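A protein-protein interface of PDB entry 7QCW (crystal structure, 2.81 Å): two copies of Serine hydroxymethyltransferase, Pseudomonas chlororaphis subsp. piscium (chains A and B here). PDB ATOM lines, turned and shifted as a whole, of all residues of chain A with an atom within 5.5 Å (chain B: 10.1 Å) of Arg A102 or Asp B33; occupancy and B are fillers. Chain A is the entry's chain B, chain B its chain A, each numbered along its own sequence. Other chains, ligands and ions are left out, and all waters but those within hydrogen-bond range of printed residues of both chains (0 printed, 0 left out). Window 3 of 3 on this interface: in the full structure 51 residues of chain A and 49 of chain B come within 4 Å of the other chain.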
ATOM      1  N   ARG A  63      32.530  -0.125 -14.185  1.00  0.00           N
ATOM      2  CA  ARG A  63      32.345  -0.440 -15.598  1.00  0.00           C
ATOM      3  C   ARG A  63      30.920  -0.133 -16.044  1.00  0.00           C
ATOM      4  O   ARG A  63      30.702   0.456 -17.109  1.00  0.00           O
ATOM      5  CB  ARG A  63      32.705  -1.908 -15.829  1.00  0.00           C
ATOM      6  CG  ARG A  63      31.983  -2.640 -16.942  1.00  0.00           C
ATOM      7  CD  ARG A  63      32.506  -4.071 -16.965  1.00  0.00           C
ATOM      8  NE  ARG A  63      31.772  -4.970 -17.847  1.00  0.00           N
ATOM      9  CZ  ARG A  63      32.057  -6.262 -17.981  1.00  0.00           C
ATOM     10  NH1 ARG A  63      33.055  -6.793 -17.285  1.00  0.00           N
ATOM     11  NH2 ARG A  63      31.348  -7.025 -18.801  1.00  0.00           N
ATOM     12  N   SER A  97      19.919  -4.717 -28.575  1.00  0.00           N
ATOM     13  CA  SER A  97      20.021  -6.131 -28.917  1.00  0.00           C
ATOM     14  C   SER A  97      21.064  -6.839 -28.058  1.00  0.00           C
ATOM     15  O   SER A  97      20.864  -7.993 -27.658  1.00  0.00           O
ATOM     16  CB  SER A  97      20.352  -6.283 -30.401  1.00  0.00           C
ATOM     17  OG  SER A  97      19.327  -5.730 -31.209  1.00  0.00           O
ATOM     18  N   LEU A  98      22.181  -6.168 -27.765  1.00  0.00           N
ATOM     19  CA  LEU A  98      23.180  -6.751 -26.875  1.00  0.00           C
ATOM     20  C   LEU A  98      22.593  -7.010 -25.492  1.00  0.00           C
ATOM     21  O   LEU A  98      22.849  -8.057 -24.886  1.00  0.00           O
ATOM     22  CB  LEU A  98      24.399  -5.831 -26.782  1.00  0.00           C
ATOM     23  CG  LEU A  98      25.623  -6.331 -26.009  1.00  0.00           C
ATOM     24  CD1 LEU A  98      26.042  -7.715 -26.483  1.00  0.00           C
ATOM     25  CD2 LEU A  98      26.774  -5.346 -26.136  1.00  0.00           C
ATOM     26  N   ALA A  99      21.804  -6.065 -24.978  1.00  0.00           N
ATOM     27  CA  ALA A  99      21.155  -6.261 -23.686  1.00  0.00           C
ATOM     28  C   ALA A  99      20.122  -7.381 -23.739  1.00  0.00           C
ATOM     29  O   ALA A  99      19.999  -8.159 -22.786  1.00  0.00           O
ATOM     30  CB  ALA A  99      20.515  -4.956 -23.214  1.00  0.00           C
ATOM     31  N   ILE A 100      19.362  -7.480 -24.835  1.00  0.00           N
ATOM     32  CA  ILE A 100      18.372  -8.553 -24.947  1.00  0.00           C
ATOM     33  C   ILE A 100      19.059  -9.911 -24.940  1.00  0.00           C
ATOM     34  O   ILE A 100      18.655 -10.829 -24.216  1.00  0.00           O
ATOM     35  CB  ILE A 100      17.506  -8.382 -26.210  1.00  0.00           C
ATOM     36  CG1 ILE A 100      17.056  -6.934 -26.392  1.00  0.00           C
ATOM     37  CG2 ILE A 100      16.296  -9.306 -26.152  1.00  0.00           C
ATOM     38  CD1 ILE A 100      15.986  -6.491 -25.432  1.00  0.00           C
ATOM     39  N   GLN A 101      20.112 -10.058 -25.746  1.00  0.00           N
ATOM     40  CA  GLN A 101      20.773 -11.353 -25.874  1.00  0.00           C
ATOM     41  C   GLN A 101      21.504 -11.731 -24.591  1.00  0.00           C
ATOM     42  O   GLN A 101      21.519 -12.906 -24.202  1.00  0.00           O
ATOM     43  CB  GLN A 101      21.723 -11.330 -27.073  1.00  0.00           C
ATOM     44  CG  GLN A 101      22.630 -12.541 -27.204  1.00  0.00           C
ATOM     45  CD  GLN A 101      24.076 -12.221 -26.886  1.00  0.00           C
ATOM     46  OE1 GLN A 101      24.565 -11.134 -27.195  1.00  0.00           O
ATOM     47  NE2 GLN A 101      24.774 -13.174 -26.278  1.00  0.00           N
ATOM     48  N   ARG A 102      22.117 -10.752 -23.920  1.00  0.00           N
ATOM     49  CA  ARG A 102      22.756 -11.028 -22.638  1.00  0.00           C
ATOM     50  C   ARG A 102      21.730 -11.412 -21.579  1.00  0.00           C
ATOM     51  O   ARG A 102      21.944 -12.357 -20.811  1.00  0.00           O
ATOM     52  CB  ARG A 102      23.576  -9.817 -22.191  1.00  0.00           C
ATOM     53  CG  ARG A 102      24.872  -9.671 -22.968  1.00  0.00           C
ATOM     54  CD  ARG A 102      25.680  -8.454 -22.554  1.00  0.00           C
ATOM     55  NE  ARG A 102      26.977  -8.454 -23.222  1.00  0.00           N
ATOM     56  CZ  ARG A 102      27.919  -7.533 -23.048  1.00  0.00           C
ATOM     57  NH1 ARG A 102      27.718  -6.516 -22.221  1.00  0.00           N
ATOM     58  NH2 ARG A 102      29.066  -7.628 -23.707  1.00  0.00           N
ATOM     59  N   ALA A 103      20.604 -10.694 -21.526  1.00  0.00           N
ATOM     60  CA  ALA A 103      19.573 -11.004 -20.541  1.00  0.00           C
ATOM     61  C   ALA A 103      18.981 -12.388 -20.777  1.00  0.00           C
ATOM     62  O   ALA A 103      18.710 -13.126 -19.823  1.00  0.00           O
ATOM     63  CB  ALA A 103      18.477  -9.941 -20.572  1.00  0.00           C
ATOM     64  N   ARG A 104      18.765 -12.751 -22.042  1.00  0.00           N
ATOM     65  CA  ARG A 104      18.189 -14.055 -22.350  1.00  0.00           C
ATOM     66  C   ARG A 104      19.132 -15.186 -21.960  1.00  0.00           C
ATOM     67  O   ARG A 104      18.693 -16.209 -21.422  1.00  0.00           O
ATOM     68  CB  ARG A 104      17.843 -14.133 -23.834  1.00  0.00           C
ATOM     69  CG  ARG A 104      16.634 -13.307 -24.226  1.00  0.00           C
ATOM     70  CD  ARG A 104      16.229 -13.621 -25.644  1.00  0.00           C
ATOM     71  NE  ARG A 104      16.118 -15.061 -25.841  1.00  0.00           N
ATOM     72  CZ  ARG A 104      15.865 -15.639 -27.008  1.00  0.00           C
ATOM     73  NH1 ARG A 104      15.699 -14.898 -28.095  1.00  0.00           N
ATOM     74  NH2 ARG A 104      15.781 -16.959 -27.089  1.00  0.00           N
ATOM     75  N   GLU A 105      20.429 -15.026 -22.227  1.00  0.00           N
ATOM     76  CA  GLU A 105      21.384 -16.060 -21.848  1.00  0.00           C
ATOM     77  C   GLU A 105      21.631 -16.081 -20.349  1.00  0.00           C
ATOM     78  O   GLU A 105      21.882 -17.150 -19.780  1.00  0.00           O
ATOM     79  CB  GLU A 105      22.710 -15.860 -22.578  1.00  0.00           C
ATOM     80  CG  GLU A 105      22.657 -16.142 -24.058  1.00  0.00           C
ATOM     81  CD  GLU A 105      23.986 -16.631 -24.590  1.00  0.00           C
ATOM     82  OE1 GLU A 105      24.877 -16.939 -23.769  1.00  0.00           O
ATOM     83  OE2 GLU A 105      24.140 -16.708 -25.826  1.00  0.00           O
ATOM     84  N   LEU A 106      21.585 -14.920 -19.696  1.00  0.00           N
ATOM     85  CA  LEU A 106      21.979 -14.879 -18.297  1.00  0.00           C
ATOM     86  C   LEU A 106      20.955 -15.614 -17.437  1.00  0.00           C
ATOM     87  O   LEU A 106      21.323 -16.376 -16.534  1.00  0.00           O
ATOM     88  CB  LEU A 106      22.136 -13.429 -17.839  1.00  0.00           C
ATOM     89  CG  LEU A 106      22.976 -13.229 -16.573  1.00  0.00           C
ATOM     90  CD1 LEU A 106      23.506 -11.819 -16.498  1.00  0.00           C
ATOM     91  CD2 LEU A 106      22.289 -13.610 -15.310  1.00  0.00           C
ATOM     92  N   PHE A 107      19.667 -15.413 -17.719  1.00  0.00           N
ATOM     93  CA  PHE A 107      18.582 -16.035 -16.974  1.00  0.00           C
ATOM     94  C   PHE A 107      17.975 -17.235 -17.689  1.00  0.00           C
ATOM     95  O   PHE A 107      17.046 -17.849 -17.158  1.00  0.00           O
ATOM     96  CB  PHE A 107      17.485 -15.003 -16.688  1.00  0.00           C
ATOM     97  CG  PHE A 107      17.930 -13.871 -15.806  1.00  0.00           C
ATOM     98  CD1 PHE A 107      17.951 -14.015 -14.429  1.00  0.00           C
ATOM     99  CD2 PHE A 107      18.333 -12.665 -16.356  1.00  0.00           C
ATOM    100  CE1 PHE A 107      18.360 -12.975 -13.616  1.00  0.00           C
ATOM    101  CE2 PHE A 107      18.745 -11.622 -15.549  1.00  0.00           C
ATOM    102  CZ  PHE A 107      18.759 -11.777 -14.177  1.00  0.00           C
ATOM    103  N   ALA A 302      23.440  -3.419 -20.324  1.00  0.00           N
ATOM    104  CA  ALA A 302      24.231  -4.385 -21.074  1.00  0.00           C
ATOM    105  C   ALA A 302      25.543  -4.676 -20.358  1.00  0.00           C
ATOM    106  O   ALA A 302      25.950  -5.837 -20.226  1.00  0.00           O
ATOM    107  CB  ALA A 302      24.485  -3.865 -22.488  1.00  0.00           C
ATOM    108  N   ALA A 303      26.215  -3.629 -19.874  1.00  0.00           N
ATOM    109  CA  ALA A 303      27.441  -3.829 -19.111  1.00  0.00           C
ATOM    110  C   ALA A 303      27.171  -4.612 -17.833  1.00  0.00           C
ATOM    111  O   ALA A 303      27.945  -5.506 -17.469  1.00  0.00           O
ATOM    112  CB  ALA A 303      28.088  -2.482 -18.792  1.00  0.00           C
ATOM    113  N   LEU A 305      24.631  -6.717 -17.216  1.00  0.00           N
ATOM    114  CA  LEU A 305      24.319  -8.091 -17.600  1.00  0.00           C
ATOM    115  C   LEU A 305      25.572  -8.859 -18.004  1.00  0.00           C
ATOM    116  O   LEU A 305      25.694 -10.053 -17.713  1.00  0.00           O
ATOM    117  CB  LEU A 305      23.284  -8.086 -18.727  1.00  0.00           C
ATOM    118  CG  LEU A 305      21.793  -8.135 -18.367  1.00  0.00           C
ATOM    119  CD1 LEU A 305      21.433  -9.511 -17.879  1.00  0.00           C
ATOM    120  CD2 LEU A 305      21.469  -7.146 -17.258  1.00  0.00           C
ATOM    121  N   GLY A 306      26.511  -8.200 -18.683  1.00  0.00           N
ATOM    122  CA  GLY A 306      27.744  -8.876 -19.054  1.00  0.00           C
ATOM    123  C   GLY A 306      28.576  -9.269 -17.849  1.00  0.00           C
ATOM    124  O   GLY A 306      29.081 -10.393 -17.767  1.00  0.00           O
ATOM    125  N   MET A 309      27.596 -12.387 -15.980  1.00  0.00           N
ATOM    126  CA  MET A 309      28.002 -13.601 -16.675  1.00  0.00           C
ATOM    127  C   MET A 309      29.444 -13.966 -16.335  1.00  0.00           C
ATOM    128  O   MET A 309      29.806 -15.149 -16.359  1.00  0.00           O
ATOM    129  CB  MET A 309      27.789 -13.402 -18.185  1.00  0.00           C
ATOM    130  CG  MET A 309      26.300 -13.207 -18.542  1.00  0.00           C
ATOM    131  SD  MET A 309      25.851 -12.797 -20.245  1.00  0.00           S
ATOM    132  CE  MET A 309      26.114 -14.373 -21.046  1.00  0.00           C
ATOM    133  N   GLY B  25      36.968   3.078 -14.318  1.00  0.00           N
ATOM    134  CA  GLY B  25      35.766   2.399 -14.775  1.00  0.00           C
ATOM    135  C   GLY B  25      35.663   2.360 -16.285  1.00  0.00           C
ATOM    136  O   GLY B  25      35.204   1.370 -16.862  1.00  0.00           O
ATOM    137  N   LEU B  26      36.106   3.433 -16.943  1.00  0.00           N
ATOM    138  CA  LEU B  26      36.262   3.386 -18.389  1.00  0.00           C
ATOM    139  C   LEU B  26      37.284   2.336 -18.773  1.00  0.00           C
ATOM    140  O   LEU B  26      37.127   1.646 -19.784  1.00  0.00           O
ATOM    141  CB  LEU B  26      36.676   4.752 -18.933  1.00  0.00           C
ATOM    142  CG  LEU B  26      35.646   5.884 -18.969  1.00  0.00           C
ATOM    143  CD1 LEU B  26      36.343   7.235 -19.015  1.00  0.00           C
ATOM    144  CD2 LEU B  26      34.705   5.721 -20.155  1.00  0.00           C
ATOM    145  N   ALA B  27      38.342   2.206 -17.968  1.00  0.00           N
ATOM    146  CA  ALA B  27      39.388   1.231 -18.241  1.00  0.00           C
ATOM    147  C   ALA B  27      38.890  -0.200 -18.080  1.00  0.00           C
ATOM    148  O   ALA B  27      39.363  -1.096 -18.785  1.00  0.00           O
ATOM    149  CB  ALA B  27      40.583   1.487 -17.324  1.00  0.00           C
ATOM    150  N   ASP B  28      37.954  -0.442 -17.157  1.00  0.00           N
ATOM    151  CA  ASP B  28      37.392  -1.784 -17.028  1.00  0.00           C
ATOM    152  C   ASP B  28      36.576  -2.159 -18.258  1.00  0.00           C
ATOM    153  O   ASP B  28      36.654  -3.296 -18.738  1.00  0.00           O
ATOM    154  CB  ASP B  28      36.530  -1.889 -15.768  1.00  0.00           C
ATOM    155  CG  ASP B  28      37.268  -1.465 -14.517  1.00  0.00           C
ATOM    156  OD1 ASP B  28      38.467  -1.794 -14.392  1.00  0.00           O
ATOM    157  OD2 ASP B  28      36.647  -0.813 -13.652  1.00  0.00           O
ATOM    158  N   LEU B  29      35.785  -1.217 -18.777  1.00  0.00           N
ATOM    159  CA  LEU B  29      35.001  -1.484 -19.978  1.00  0.00           C
ATOM    160  C   LEU B  29      35.904  -1.769 -21.172  1.00  0.00           C
ATOM    161  O   LEU B  29      35.640  -2.690 -21.952  1.00  0.00           O
ATOM    162  CB  LEU B  29      34.078  -0.300 -20.272  1.00  0.00           C
ATOM    163  CG  LEU B  29      32.933  -0.510 -21.266  1.00  0.00           C
ATOM    164  CD1 LEU B  29      31.804  -1.306 -20.631  1.00  0.00           C
ATOM    165  CD2 LEU B  29      32.425   0.825 -21.790  1.00  0.00           C
ATOM    166  N   GLN B  30      36.987  -1.001 -21.317  1.00  0.00           N
ATOM    167  CA  GLN B  30      37.871  -1.168 -22.466  1.00  0.00           C
ATOM    168  C   GLN B  30      38.481  -2.564 -22.516  1.00  0.00           C
ATOM    169  O   GLN B  30      38.700  -3.108 -23.604  1.00  0.00           O
ATOM    170  CB  GLN B  30      38.978  -0.113 -22.428  1.00  0.00           C
ATOM    171  CG  GLN B  30      38.531   1.296 -22.797  1.00  0.00           C
ATOM    172  CD  GLN B  30      38.295   1.489 -24.286  1.00  0.00           C
ATOM    173  OE1 GLN B  30      38.162   0.527 -25.043  1.00  0.00           O
ATOM    174  NE2 GLN B  30      38.247   2.746 -24.714  1.00  0.00           N
ATOM    175  N   GLU B  31      38.757  -3.157 -21.356  1.00  0.00           N
ATOM    176  CA  GLU B  31      39.441  -4.442 -21.278  1.00  0.00           C
ATOM    177  C   GLU B  31      38.481  -5.625 -21.281  1.00  0.00           C
ATOM    178  O   GLU B  31      38.770  -6.654 -21.901  1.00  0.00           O
ATOM    179  CB  GLU B  31      40.297  -4.494 -20.012  1.00  0.00           C
ATOM    180  CG  GLU B  31      41.255  -3.331 -19.859  1.00  0.00           C
ATOM    181  CD  GLU B  31      41.868  -3.272 -18.476  1.00  0.00           C
ATOM    182  OE1 GLU B  31      41.643  -4.214 -17.686  1.00  0.00           O
ATOM    183  OE2 GLU B  31      42.557  -2.277 -18.169  1.00  0.00           O
ATOM    184  N   HIS B  32      37.343  -5.503 -20.597  1.00  0.00           N
ATOM    185  CA  HIS B  32      36.467  -6.640 -20.348  1.00  0.00           C
ATOM    186  C   HIS B  32      35.177  -6.620 -21.152  1.00  0.00           C
ATOM    187  O   HIS B  32      34.682  -7.690 -21.516  1.00  0.00           O
ATOM    188  CB  HIS B  32      36.131  -6.725 -18.856  1.00  0.00           C
ATOM    189  CG  HIS B  32      37.339  -6.770 -17.974  1.00  0.00           C
ATOM    190  ND1 HIS B  32      38.259  -7.794 -18.027  1.00  0.00           N
ATOM    191  CD2 HIS B  32      37.788  -5.911 -17.028  1.00  0.00           C
ATOM    192  CE1 HIS B  32      39.217  -7.569 -17.146  1.00  0.00           C
ATOM    193  NE2 HIS B  32      38.955  -6.433 -16.527  1.00  0.00           N
ATOM    194  N   ASP B  33      34.610  -5.449 -21.426  1.00  0.00           N
ATOM    195  CA  ASP B  33      33.464  -5.326 -22.325  1.00  0.00           C
ATOM    196  C   ASP B  33      33.888  -4.416 -23.471  1.00  0.00           C
ATOM    197  O   ASP B  33      33.538  -3.234 -23.514  1.00  0.00           O
ATOM    198  CB  ASP B  33      32.238  -4.780 -21.578  1.00  0.00           C
ATOM    199  CG  ASP B  33      30.933  -5.325 -22.121  1.00  0.00           C
ATOM    200  OD1 ASP B  33      30.926  -5.840 -23.260  1.00  0.00           O
ATOM    201  OD2 ASP B  33      29.912  -5.242 -21.406  1.00  0.00           O
ATOM    202  N   ALA B  34      34.620  -4.984 -24.428  1.00  0.00           N
ATOM    203  CA  ALA B  34      35.131  -4.198 -25.540  1.00  0.00           C
ATOM    204  C   ALA B  34      34.098  -4.095 -26.646  1.00  0.00           C
ATOM    205  O   ALA B  34      33.905  -3.022 -27.214  1.00  0.00           O
ATOM    206  CB  ALA B  34      36.428  -4.810 -26.074  1.00  0.00           C
ATOM    207  N   GLU B  35      33.414  -5.200 -26.934  1.00  0.00           N
ATOM    208  CA  GLU B  35      32.190  -5.197 -27.731  1.00  0.00           C
ATOM    209  C   GLU B  35      31.232  -4.052 -27.424  1.00  0.00           C
ATOM    210  O   GLU B  35      30.891  -3.266 -28.321  1.00  0.00           O
ATOM    211  CB  GLU B  35      31.565  -6.611 -27.626  1.00  0.00           C
ATOM    212  CG  GLU B  35      30.081  -6.918 -27.994  1.00  0.00           C
ATOM    213  CD  GLU B  35      29.559  -6.362 -29.307  1.00  0.00           C
ATOM    214  OE1 GLU B  35      30.351  -5.867 -30.127  1.00  0.00           O
ATOM    215  OE2 GLU B  35      28.325  -6.545 -29.522  1.00  0.00           O
ATOM    216  N   LEU B  36      30.819  -3.904 -26.175  1.00  0.00           N
ATOM    217  CA  LEU B  36      29.964  -2.767 -25.866  1.00  0.00           C
ATOM    218  C   LEU B  36      30.669  -1.447 -26.195  1.00  0.00           C
ATOM    219  O   LEU B  36      30.049  -0.525 -26.739  1.00  0.00           O
ATOM    220  CB  LEU B  36      29.522  -2.814 -24.403  1.00  0.00           C
ATOM    221  CG  LEU B  36      28.545  -1.701 -24.018  1.00  0.00           C
ATOM    222  CD1 LEU B  36      27.139  -2.071 -24.464  1.00  0.00           C
ATOM    223  CD2 LEU B  36      28.593  -1.459 -22.530  1.00  0.00           C
ATOM    224  N   ALA B  37      31.985  -1.375 -25.964  1.00  0.00           N
ATOM    225  CA  ALA B  37      32.709  -0.112 -26.126  1.00  0.00           C
ATOM    226  C   ALA B  37      32.791   0.329 -27.589  1.00  0.00           C
ATOM    227  O   ALA B  37      32.861   1.533 -27.876  1.00  0.00           O
ATOM    228  CB  ALA B  37      34.112  -0.231 -25.520  1.00  0.00           C
ATOM    229  N   ARG B  38      32.775  -0.618 -28.532  1.00  0.00           N
ATOM    230  CA  ARG B  38      32.757  -0.229 -29.938  1.00  0.00           C
ATOM    231  C   ARG B  38      31.494   0.557 -30.271  1.00  0.00           C
ATOM    232  O   ARG B  38      31.570   1.616 -30.901  1.00  0.00           O
ATOM    233  CB  ARG B  38      32.909  -1.446 -30.857  1.00  0.00           C
ATOM    234  CG  ARG B  38      34.375  -1.923 -31.006  1.00  0.00           C
ATOM    235  CD  ARG B  38      34.799  -2.815 -29.865  1.00  0.00           C
ATOM    236  NE  ARG B  38      36.225  -3.194 -29.746  1.00  0.00           N
ATOM    237  CZ  ARG B  38      36.792  -4.276 -30.275  1.00  0.00           C
ATOM    238  NH1 ARG B  38      36.063  -5.120 -31.007  1.00  0.00           N
ATOM    239  NH2 ARG B  38      38.080  -4.516 -30.048  1.00  0.00           N
ATOM    240  N   ILE B  39      30.331   0.081 -29.817  1.00  0.00           N
ATOM    241  CA  ILE B  39      29.080   0.789 -30.089  1.00  0.00           C
ATOM    242  C   ILE B  39      29.069   2.153 -29.404  1.00  0.00           C
ATOM    243  O   ILE B  39      28.570   3.140 -29.959  1.00  0.00           O
ATOM    244  CB  ILE B  39      27.866  -0.061 -29.667  1.00  0.00           C
ATOM    245  CG1 ILE B  39      27.746  -1.338 -30.510  1.00  0.00           C
ATOM    246  CG2 ILE B  39      26.604   0.741 -29.816  1.00  0.00           C
ATOM    247  CD1 ILE B  39      28.440  -2.553 -29.966  1.00  0.00           C
ATOM    248  N   LEU B  40      29.614   2.232 -28.190  1.00  0.00           N
ATOM    249  CA  LEU B  40      29.647   3.514 -27.498  1.00  0.00           C
ATOM    250  C   LEU B  40      30.520   4.515 -28.242  1.00  0.00           C
ATOM    251  O   LEU B  40      30.169   5.696 -28.351  1.00  0.00           O
ATOM    252  CB  LEU B  40      30.137   3.332 -26.061  1.00  0.00           C
ATOM    253  CG  LEU B  40      29.069   2.893 -25.056  1.00  0.00           C
ATOM    254  CD1 LEU B  40      28.013   3.935 -25.037  1.00  0.00           C
ATOM    255  CD2 LEU B  40      28.443   1.551 -25.352  1.00  0.00           C
ATOM    256  N   ASP B  41      31.660   4.059 -28.764  1.00  0.00           N
ATOM    257  CA  ASP B  41      32.519   4.931 -29.555  1.00  0.00           C
ATOM    258  C   ASP B  41      31.902   5.247 -30.912  1.00  0.00           C
ATOM    259  O   ASP B  41      32.100   6.346 -31.441  1.00  0.00           O
ATOM    260  CB  ASP B  41      33.894   4.287 -29.733  1.00  0.00           C
ATOM    261  CG  ASP B  41      34.792   4.491 -28.529  1.00  0.00           C
ATOM    262  OD1 ASP B  41      34.437   5.303 -27.650  1.00  0.00           O
ATOM    263  OD2 ASP B  41      35.852   3.833 -28.459  1.00  0.00           O
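Printed residues of chain B within 4 Å of Arg A63: Gly B25 (3.6 Å), Asp B28 (3.8 Å), Leu B29 (3.9 Å), His B32 (3.5 Å) and Asp B33 (3.5 Å). Leu A98 touches just these residues of chain B: Glu B35 and Leu B36. No residue of chain B comes within 4 Å of Ala A99. Ile A100 touches none of the printed residues of chain B. No residue of chain B comes within 4 Å of Gln A101. Of chain B, only Asp B33 (2.6 Å) comes within 4 Å of Arg A102. Ala A103 touches none of the printed residues of chain B. No residue of chain B comes within 4 Å of Leu A106. Of the printed residues of chain B, Ala A303 touches Asp B33 (3.7 Å) and Leu B36 (3.9 Å). Met A309 touches none of the printed residues of chain B. Of the printed residues of chain A, Asp B28 touches Arg A63 (3.8 Å). Of the printed residues of chain A, His B32 touches Arg A63. Asp B33 touches three residues of chain A. Of the printed residues of chain A, Glu B35 touches Leu A98. Of the printed residues of chain A, Leu B36 touches Leu A98 (3.7 Å), Ala A302 (3.8 Å) and Ala A303 (3.9 Å). The nearest printed residue of chain A that does not touch Asp B28 is Ala A303 (8.5 Å).
No position is printed for both chains.
Among the printed residues, pairs that only touch across the chains: Arg A63 with Gly B25, Arg A63 with Asp B28, Arg A63 with Leu B29, Arg A63 with His B32, Leu A98 with Glu B35, Leu A98 with Leu B36, Ala A302 with Leu B36, Ala A303 with Asp B33 and Ala A303 with Leu B36.
NH1 of Arg A102 is in hydrogen-bond range of O of Ala A302 (2.8 Å).
Of the 17 printed residues of chain B, 7 touch a printed residue of chain A. Of the 17 printed residues of chain A, 5 touch a printed residue of chain B. Printed residues of chain A that touch a printed residue of chain B: Arg A63, Leu A98, Arg A102, Ala A302 and Ala A303. Hydrophobic or aromatic side chains of chain A within 4 Å of the printed part of chain B: Leu A98, Ala A302 and Ala A303. Among the printed residues, 11 pairs touch across the chains.
The guanidinium group (NH2) of Arg A63 lies within salt-bridge range of the side-chain carboxylate (OD2) of Asp B33 (3.5 Å). OD1 of Asp B33 is in salt-bridge range of NH2 of Arg A102 (2.6 Å).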
